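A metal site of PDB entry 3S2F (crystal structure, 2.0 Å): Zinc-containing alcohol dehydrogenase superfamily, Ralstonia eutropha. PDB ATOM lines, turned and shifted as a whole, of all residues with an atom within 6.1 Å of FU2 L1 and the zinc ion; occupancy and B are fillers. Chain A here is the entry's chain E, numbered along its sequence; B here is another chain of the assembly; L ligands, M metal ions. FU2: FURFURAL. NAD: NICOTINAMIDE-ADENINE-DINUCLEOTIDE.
The side-chain carboxylate (OD1) of Asp 43 lies close to a ring nitrogen (ND1) of His 63 (3.4 Å). OD2 of Asp 43 is in hydrogen-bond range of N of Cys 40 (3.0 Å). The side-chain sulfur (SG) of Cys 40 lies close to the guanidinium group (NH1) of Arg 333, 3.4 Å away. The backbone NH of Thr 42 lies close to the side-chain sulfur of Cys 40 (3.4 Å). The side-chain hydroxyl (OG1) of Thr 154 is in hydrogen-bond range of the backbone carbonyl oxygen (O) of Cys 150 (2.7 Å).
NE2 of His 63 binds the zinc ion. The zinc ion is bound by an oxygen (OXT) of FU2 L1. The side-chain sulfur (SG) of Cys 40 binds the zinc ion (2.4 Å). The zinc ion is bound by the side-chain sulfur (SG) of Cys 150 (2.4 Å).
An oxygen (O2N) of NAD L2 lies within hydrogen-bond range of the backbone NH of His 41, at 3.3 Å. O2D of NAD L2 sits at hydrogen-bond distance from OG1 of Thr 42. NH2 of Arg 333 lies within salt-bridge range of O2N of NAD L2 (2.8 Å). O1N of NAD L2 is in hydrogen-bond range of N of Leu 178 (3.0 Å). N of Val 288 sits at hydrogen-bond distance from O7N of NAD L2, at 2.5 Å. OG1 of Thr 42 is in hydrogen-bond range of O3 of FU2 L1 (3.2 Å).
Of the 18 residues printed, 3 come within 4 Å of the zinc ion.
Residues that only touch FU2 L1: Trp 51, Trp 89, Leu 264, Ile 287 and Val 288. Hydrophobic or aromatic side chains that line FU2 L1: Trp 51, His 63, Trp 89, Leu 264, Ile 287 and Val 288. Nine residues have an atom within 4 Å of FU2 L1: Cys 40, Thr 42, Trp 51, His 63, Trp 89, Cys 150, Leu 264, Ile 287 and Val 288.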
ATOM      1  N   CYS A  40      32.320   2.504 -10.457  1.00  0.00           N
ATOM      2  CA  CYS A  40      31.811   1.273  -9.865  1.00  0.00           C
ATOM      3  C   CYS A  40      32.347   0.059 -10.607  1.00  0.00           C
ATOM      4  O   CYS A  40      32.581   0.106 -11.820  1.00  0.00           O
ATOM      5  CB  CYS A  40      30.277   1.259  -9.879  1.00  0.00           C
ATOM      6  SG  CYS A  40      29.592  -0.224  -9.116  1.00  0.00           S
ATOM      7  N   HIS A  41      32.538  -1.037  -9.883  1.00  0.00           N
ATOM      8  CA  HIS A  41      33.047  -2.256 -10.480  1.00  0.00           C
ATOM      9  C   HIS A  41      32.135  -2.680 -11.630  1.00  0.00           C
ATOM     10  O   HIS A  41      32.594  -3.272 -12.608  1.00  0.00           O
ATOM     11  CB  HIS A  41      33.133  -3.359  -9.451  1.00  0.00           C
ATOM     12  CG  HIS A  41      34.085  -4.465  -9.825  1.00  0.00           C
ATOM     13  ND1 HIS A  41      33.833  -5.349 -10.848  1.00  0.00           N
ATOM     14  CD2 HIS A  41      35.289  -4.803  -9.309  1.00  0.00           C
ATOM     15  CE1 HIS A  41      34.838  -6.193 -10.944  1.00  0.00           C
ATOM     16  NE2 HIS A  41      35.743  -5.889 -10.026  1.00  0.00           N
ATOM     17  N   THR A  42      30.848  -2.380 -11.492  1.00  0.00           N
ATOM     18  CA  THR A  42      29.873  -2.674 -12.527  1.00  0.00           C
ATOM     19  C   THR A  42      30.296  -2.084 -13.861  1.00  0.00           C
ATOM     20  O   THR A  42      30.030  -2.660 -14.922  1.00  0.00           O
ATOM     21  CB  THR A  42      28.480  -2.131 -12.145  1.00  0.00           C
ATOM     22  OG1 THR A  42      27.875  -3.004 -11.186  1.00  0.00           O
ATOM     23  CG2 THR A  42      27.593  -2.041 -13.377  1.00  0.00           C
ATOM     24  N   ASP A  43      30.950  -0.930 -13.809  1.00  0.00           N
ATOM     25  CA  ASP A  43      31.365  -0.226 -15.018  1.00  0.00           C
ATOM     26  C   ASP A  43      32.330  -1.057 -15.847  1.00  0.00           C
ATOM     27  O   ASP A  43      32.339  -0.968 -17.079  1.00  0.00           O
ATOM     28  CB  ASP A  43      31.999   1.116 -14.662  1.00  0.00           C
ATOM     29  CG  ASP A  43      31.032   2.056 -13.953  1.00  0.00           C
ATOM     30  OD1 ASP A  43      29.807   1.860 -14.092  1.00  0.00           O
ATOM     31  OD2 ASP A  43      31.500   2.982 -13.259  1.00  0.00           O
ATOM     32  N   TRP A  51      27.843  -9.221 -19.728  1.00  0.00           N
ATOM     33  CA  TRP A  51      26.712  -9.667 -18.909  1.00  0.00           C
ATOM     34  C   TRP A  51      25.621 -10.210 -19.824  1.00  0.00           C
ATOM     35  O   TRP A  51      25.599  -9.878 -21.010  1.00  0.00           O
ATOM     36  CB  TRP A  51      26.166  -8.508 -18.065  1.00  0.00           C
ATOM     37  CG  TRP A  51      26.948  -8.228 -16.808  1.00  0.00           C
ATOM     38  CD1 TRP A  51      28.039  -8.915 -16.337  1.00  0.00           C
ATOM     39  CD2 TRP A  51      26.709  -7.177 -15.865  1.00  0.00           C
ATOM     40  NE1 TRP A  51      28.479  -8.356 -15.166  1.00  0.00           N
ATOM     41  CE2 TRP A  51      27.682  -7.290 -14.847  1.00  0.00           C
ATOM     42  CE3 TRP A  51      25.755  -6.150 -15.776  1.00  0.00           C
ATOM     43  CZ2 TRP A  51      27.729  -6.406 -13.771  1.00  0.00           C
ATOM     44  CZ3 TRP A  51      25.814  -5.281 -14.706  1.00  0.00           C
ATOM     45  CH2 TRP A  51      26.792  -5.419 -13.714  1.00  0.00           C
ATOM     46  N   HIS A  63      27.390   5.664 -13.209  1.00  0.00           N
ATOM     47  CA  HIS A  63      26.154   5.866 -12.461  1.00  0.00           C
ATOM     48  C   HIS A  63      26.409   6.333 -11.030  1.00  0.00           C
ATOM     49  O   HIS A  63      25.616   6.060 -10.128  1.00  0.00           O
ATOM     50  CB  HIS A  63      25.283   4.613 -12.478  1.00  0.00           C
ATOM     51  CG  HIS A  63      26.014   3.374 -12.057  1.00  0.00           C
ATOM     52  ND1 HIS A  63      26.709   2.586 -12.960  1.00  0.00           N
ATOM     53  CD2 HIS A  63      26.150   2.783 -10.850  1.00  0.00           C
ATOM     54  CE1 HIS A  63      27.246   1.570 -12.323  1.00  0.00           C
ATOM     55  NE2 HIS A  63      26.928   1.666 -11.033  1.00  0.00           N
ATOM     56  N   GLU A  64      27.535   7.013 -10.834  1.00  0.00           N
ATOM     57  CA  GLU A  64      27.818   7.675  -9.570  1.00  0.00           C
ATOM     58  C   GLU A  64      28.201   9.115  -9.853  1.00  0.00           C
ATOM     59  O   GLU A  64      29.008   9.720  -9.139  1.00  0.00           O
ATOM     60  CB  GLU A  64      28.928   6.963  -8.800  1.00  0.00           C
ATOM     61  CG  GLU A  64      28.532   5.599  -8.285  1.00  0.00           C
ATOM     62  CD  GLU A  64      29.513   5.063  -7.262  1.00  0.00           C
ATOM     63  OE1 GLU A  64      30.689   5.477  -7.297  1.00  0.00           O
ATOM     64  OE2 GLU A  64      29.103   4.247  -6.404  1.00  0.00           O
ATOM     65  N   TRP A  89      22.229   4.384 -10.652  1.00  0.00           N
ATOM     66  CA  TRP A  89      21.929   3.248 -11.517  1.00  0.00           C
ATOM     67  C   TRP A  89      20.487   3.268 -12.006  1.00  0.00           C
ATOM     68  O   TRP A  89      20.217   3.080 -13.199  1.00  0.00           O
ATOM     69  CB  TRP A  89      22.241   1.942 -10.777  1.00  0.00           C
ATOM     70  CG  TRP A  89      21.901   0.694 -11.527  1.00  0.00           C
ATOM     71  CD1 TRP A  89      20.889  -0.175 -11.252  1.00  0.00           C
ATOM     72  CD2 TRP A  89      22.578   0.157 -12.677  1.00  0.00           C
ATOM     73  NE1 TRP A  89      20.887  -1.211 -12.155  1.00  0.00           N
ATOM     74  CE2 TRP A  89      21.915  -1.030 -13.034  1.00  0.00           C
ATOM     75  CE3 TRP A  89      23.682   0.576 -13.427  1.00  0.00           C
ATOM     76  CZ2 TRP A  89      22.319  -1.810 -14.119  1.00  0.00           C
ATOM     77  CZ3 TRP A  89      24.075  -0.204 -14.502  1.00  0.00           C
ATOM     78  CH2 TRP A  89      23.402  -1.380 -14.840  1.00  0.00           C
ATOM     79  N   CYS A 150      25.761   4.878  -5.535  1.00  0.00           N
ATOM     80  CA  CYS A 150      25.605   3.454  -5.810  1.00  0.00           C
ATOM     81  C   CYS A 150      26.176   2.558  -4.711  1.00  0.00           C
ATOM     82  O   CYS A 150      25.466   1.701  -4.187  1.00  0.00           O
ATOM     83  CB  CYS A 150      26.189   3.069  -7.159  1.00  0.00           C
ATOM     84  SG  CYS A 150      25.730   1.390  -7.635  1.00  0.00           S
ATOM     85  N   ALA A 151      27.444   2.741  -4.377  1.00  0.00           N
ATOM     86  CA  ALA A 151      28.067   1.940  -3.333  1.00  0.00           C
ATOM     87  C   ALA A 151      27.322   2.097  -2.017  1.00  0.00           C
ATOM     88  O   ALA A 151      27.067   1.123  -1.317  1.00  0.00           O
ATOM     89  CB  ALA A 151      29.531   2.335  -3.166  1.00  0.00           C
ATOM     90  N   THR A 154      23.296   1.079  -2.160  1.00  0.00           N
ATOM     91  CA  THR A 154      23.218  -0.368  -2.362  1.00  0.00           C
ATOM     92  C   THR A 154      23.422  -1.162  -1.069  1.00  0.00           C
ATOM     93  O   THR A 154      22.583  -1.980  -0.714  1.00  0.00           O
ATOM     94  CB  THR A 154      24.230  -0.846  -3.425  1.00  0.00           C
ATOM     95  OG1 THR A 154      23.833  -0.364  -4.717  1.00  0.00           O
ATOM     96  CG2 THR A 154      24.295  -2.365  -3.450  1.00  0.00           C
ATOM     97  N   LEU A 178      31.885  -0.925  -2.340  1.00  0.00           N
ATOM     98  CA  LEU A 178      30.669  -1.133  -1.562  1.00  0.00           C
ATOM     99  C   LEU A 178      30.993  -1.547  -0.131  1.00  0.00           C
ATOM    100  O   LEU A 178      30.452  -0.983   0.816  1.00  0.00           O
ATOM    101  CB  LEU A 178      29.785  -2.203  -2.214  1.00  0.00           C
ATOM    102  CG  LEU A 178      28.768  -1.778  -3.272  1.00  0.00           C
ATOM    103  CD1 LEU A 178      29.466  -1.231  -4.496  1.00  0.00           C
ATOM    104  CD2 LEU A 178      27.865  -2.942  -3.631  1.00  0.00           C
ATOM    105  N   LEU A 264      28.272  -9.260  -8.178  1.00  0.00           N
ATOM    106  CA  LEU A 264      27.824  -9.722  -9.487  1.00  0.00           C
ATOM    107  C   LEU A 264      28.893 -10.433 -10.299  1.00  0.00           C
ATOM    108  O   LEU A 264      29.100 -10.122 -11.475  1.00  0.00           O
ATOM    109  CB  LEU A 264      27.253  -8.544 -10.296  1.00  0.00           C
ATOM    110  CG  LEU A 264      25.887  -8.038  -9.847  1.00  0.00           C
ATOM    111  CD1 LEU A 264      25.458  -6.852 -10.686  1.00  0.00           C
ATOM    112  CD2 LEU A 264      24.848  -9.151  -9.930  1.00  0.00           C
ATOM    113  N   ILE A 287      19.035  -5.356  -4.833  1.00  0.00           N
ATOM    114  CA  ILE A 287      19.370  -4.585  -6.031  1.00  0.00           C
ATOM    115  C   ILE A 287      19.326  -3.083  -5.780  1.00  0.00           C
ATOM    116  O   ILE A 287      18.262  -2.500  -5.581  1.00  0.00           O
ATOM    117  CB  ILE A 287      18.458  -4.979  -7.215  1.00  0.00           C
ATOM    118  CG1 ILE A 287      18.718  -4.072  -8.424  1.00  0.00           C
ATOM    119  CG2 ILE A 287      16.994  -4.949  -6.806  1.00  0.00           C
ATOM    120  CD1 ILE A 287      20.024  -4.375  -9.125  1.00  0.00           C
ATOM    121  N   VAL A 288      20.503  -2.455  -5.828  1.00  0.00           N
ATOM    122  CA  VAL A 288      20.699  -1.055  -5.460  1.00  0.00           C
ATOM    123  C   VAL A 288      19.718  -0.586  -4.382  1.00  0.00           C
ATOM    124  O   VAL A 288      19.585  -1.215  -3.338  1.00  0.00           O
ATOM    125  CB  VAL A 288      20.670  -0.096  -6.676  1.00  0.00           C
ATOM    126  CG1 VAL A 288      21.908  -0.302  -7.531  1.00  0.00           C
ATOM    127  CG2 VAL A 288      19.394  -0.285  -7.494  1.00  0.00           C
ATOM    128  N   ARG A 333      37.056   3.535  -2.944  1.00  0.00           N
ATOM    129  CA  ARG A 333      36.529   3.977  -4.235  1.00  0.00           C
ATOM    130  C   ARG A 333      37.488   4.914  -4.963  1.00  0.00           C
ATOM    131  O   ARG A 333      38.210   5.698  -4.342  1.00  0.00           O
ATOM    132  CB  ARG A 333      35.195   4.690  -4.026  1.00  0.00           C
ATOM    133  CG  ARG A 333      33.959   3.858  -4.331  1.00  0.00           C
ATOM    134  CD  ARG A 333      33.700   3.777  -5.828  1.00  0.00           C
ATOM    135  NE  ARG A 333      32.342   3.314  -6.107  1.00  0.00           N
ATOM    136  CZ  ARG A 333      32.017   2.053  -6.319  1.00  0.00           C
ATOM    137  NH1 ARG A 333      30.751   1.720  -6.563  1.00  0.00           N
ATOM    138  NH2 ARG A 333      32.951   1.114  -6.306  1.00  0.00           N
ATOM    139  N   PHE B 274      23.460 -13.672 -11.033  1.00  0.00           N
ATOM    140  CA  PHE B 274      22.866 -12.562 -11.765  1.00  0.00           C
ATOM    141  C   PHE B 274      21.345 -12.506 -11.635  1.00  0.00           C
ATOM    142  O   PHE B 274      20.771 -11.451 -11.369  1.00  0.00           O
ATOM    143  CB  PHE B 274      23.265 -12.632 -13.236  1.00  0.00           C
ATOM    144  CG  PHE B 274      22.890 -11.421 -14.034  1.00  0.00           C
ATOM    145  CD1 PHE B 274      23.630 -10.249 -13.926  1.00  0.00           C
ATOM    146  CD2 PHE B 274      21.807 -11.442 -14.897  1.00  0.00           C
ATOM    147  CE1 PHE B 274      23.291  -9.132 -14.663  1.00  0.00           C
ATOM    148  CE2 PHE B 274      21.462 -10.318 -15.632  1.00  0.00           C
ATOM    149  CZ  PHE B 274      22.210  -9.159 -15.513  1.00  0.00           C
ATOM    150  N   LEU B 278      19.716  -9.430  -9.450  1.00  0.00           N
ATOM    151  CA  LEU B 278      18.985  -8.453 -10.260  1.00  0.00           C
ATOM    152  C   LEU B 278      17.484  -8.507 -10.066  1.00  0.00           C
ATOM    153  O   LEU B 278      16.789  -7.495 -10.194  1.00  0.00           O
ATOM    154  CB  LEU B 278      19.333  -8.630 -11.741  1.00  0.00           C
ATOM    155  CG  LEU B 278      20.392  -7.680 -12.317  1.00  0.00           C
ATOM    156  CD1 LEU B 278      19.853  -6.257 -12.399  1.00  0.00           C
ATOM    157  CD2 LEU B 278      21.674  -7.735 -11.497  1.00  0.00           C
HETATM  158  C1  FU2 L   1      25.273  -1.374  -9.832  1.00  0.00           C
HETATM  159  C2  FU2 L   1      24.435  -2.394 -10.509  1.00  0.00           C
HETATM  160  O3  FU2 L   1      24.746  -2.922 -11.712  1.00  0.00           O
HETATM  161  C4  FU2 L   1      23.759  -3.801 -12.003  1.00  0.00           C
HETATM  162  C5  FU2 L   1      22.814  -3.837 -10.990  1.00  0.00           C
HETATM  163  C6  FU2 L   1      23.250  -2.925 -10.025  1.00  0.00           C
HETATM  164  OXT FU2 L   1      26.304  -0.970 -10.382  1.00  0.00           O
HETATM  165  PA  NAD L   2      35.245  -4.061  -5.982  1.00  0.00           P
HETATM  166  O1A NAD L   2      35.236  -2.634  -5.353  1.00  0.00           O
HETATM  167  O2A NAD L   2      36.534  -3.543  -6.673  1.00  0.00           O
HETATM  168  O5B NAD L   2      35.335  -4.629  -4.488  1.00  0.00           O
HETATM  169  C5B NAD L   2      36.142  -5.774  -4.315  1.00  0.00           C
HETATM  170  C4B NAD L   2      35.869  -6.562  -3.032  1.00  0.00           C
HETATM  171  O4B NAD L   2      35.650  -7.938  -3.252  1.00  0.00           O
HETATM  172  C3B NAD L   2      37.091  -6.473  -2.183  1.00  0.00           C
HETATM  173  O3B NAD L   2      37.916  -5.487  -2.688  1.00  0.00           O
HETATM  174  C2B NAD L   2      37.805  -7.732  -2.410  1.00  0.00           C
HETATM  175  O2B NAD L   2      39.026  -7.358  -2.940  1.00  0.00           O
HETATM  176  C1B NAD L   2      36.970  -8.436  -3.382  1.00  0.00           C
HETATM  177  N9A NAD L   2      37.133  -9.883  -3.295  1.00  0.00           N
HETATM  178  C8A NAD L   2      37.611 -10.676  -4.280  1.00  0.00           C
HETATM  179  N7A NAD L   2      37.560 -11.952  -3.932  1.00  0.00           N
HETATM  180  C5A NAD L   2      37.051 -12.042  -2.702  1.00  0.00           C
HETATM  181  C6A NAD L   2      36.775 -13.082  -1.835  1.00  0.00           C
HETATM  182  N6A NAD L   2      37.041 -14.450  -2.215  1.00  0.00           N
HETATM  183  N1A NAD L   2      36.244 -12.818  -0.634  1.00  0.00           N
HETATM  184  C2A NAD L   2      35.977 -11.560  -0.225  1.00  0.00           C
HETATM  185  N3A NAD L   2      36.235 -10.519  -1.037  1.00  0.00           N
HETATM  186  C4A NAD L   2      36.765 -10.730  -2.264  1.00  0.00           C
HETATM  187  O3  NAD L   2      33.882  -3.618  -6.683  1.00  0.00           O
HETATM  188  PN  NAD L   2      32.608  -2.985  -6.011  1.00  0.00           P
HETATM  189  O1N NAD L   2      32.807  -2.820  -4.538  1.00  0.00           O
HETATM  190  O2N NAD L   2      32.311  -1.624  -6.604  1.00  0.00           O
HETATM  191  O5D NAD L   2      31.368  -3.938  -6.269  1.00  0.00           O
HETATM  192  C5D NAD L   2      31.610  -5.245  -6.738  1.00  0.00           C
HETATM  193  C4D NAD L   2      30.282  -5.955  -6.755  1.00  0.00           C
HETATM  194  O4D NAD L   2      29.287  -5.018  -6.542  1.00  0.00           O
HETATM  195  C3D NAD L   2      30.054  -6.626  -8.051  1.00  0.00           C
HETATM  196  O3D NAD L   2      31.176  -6.442  -8.797  1.00  0.00           O
HETATM  197  C2D NAD L   2      28.940  -5.843  -8.621  1.00  0.00           C
HETATM  198  O2D NAD L   2      29.449  -4.795  -9.354  1.00  0.00           O
HETATM  199  C1D NAD L   2      28.253  -5.378  -7.390  1.00  0.00           C
HETATM  200  N1N NAD L   2      27.278  -4.301  -7.417  1.00  0.00           N
HETATM  201  C2N NAD L   2      25.963  -4.620  -7.181  1.00  0.00           C
HETATM  202  C3N NAD L   2      25.003  -3.620  -7.041  1.00  0.00           C
HETATM  203  C7N NAD L   2      23.594  -4.090  -6.795  1.00  0.00           C
HETATM  204  O7N NAD L   2      22.692  -3.289  -6.627  1.00  0.00           O
HETATM  205  N7N NAD L   2      23.321  -5.505  -6.758  1.00  0.00           N
HETATM  206  C4N NAD L   2      25.350  -2.297  -7.104  1.00  0.00           C
HETATM  207  C5N NAD L   2      26.679  -1.975  -7.325  1.00  0.00           C
HETATM  208  C6N NAD L   2      27.651  -2.980  -7.461  1.00  0.00           C
HETATM  209 ZN    ZN M   1      27.342   0.610  -9.239  1.00  0.00          ZN
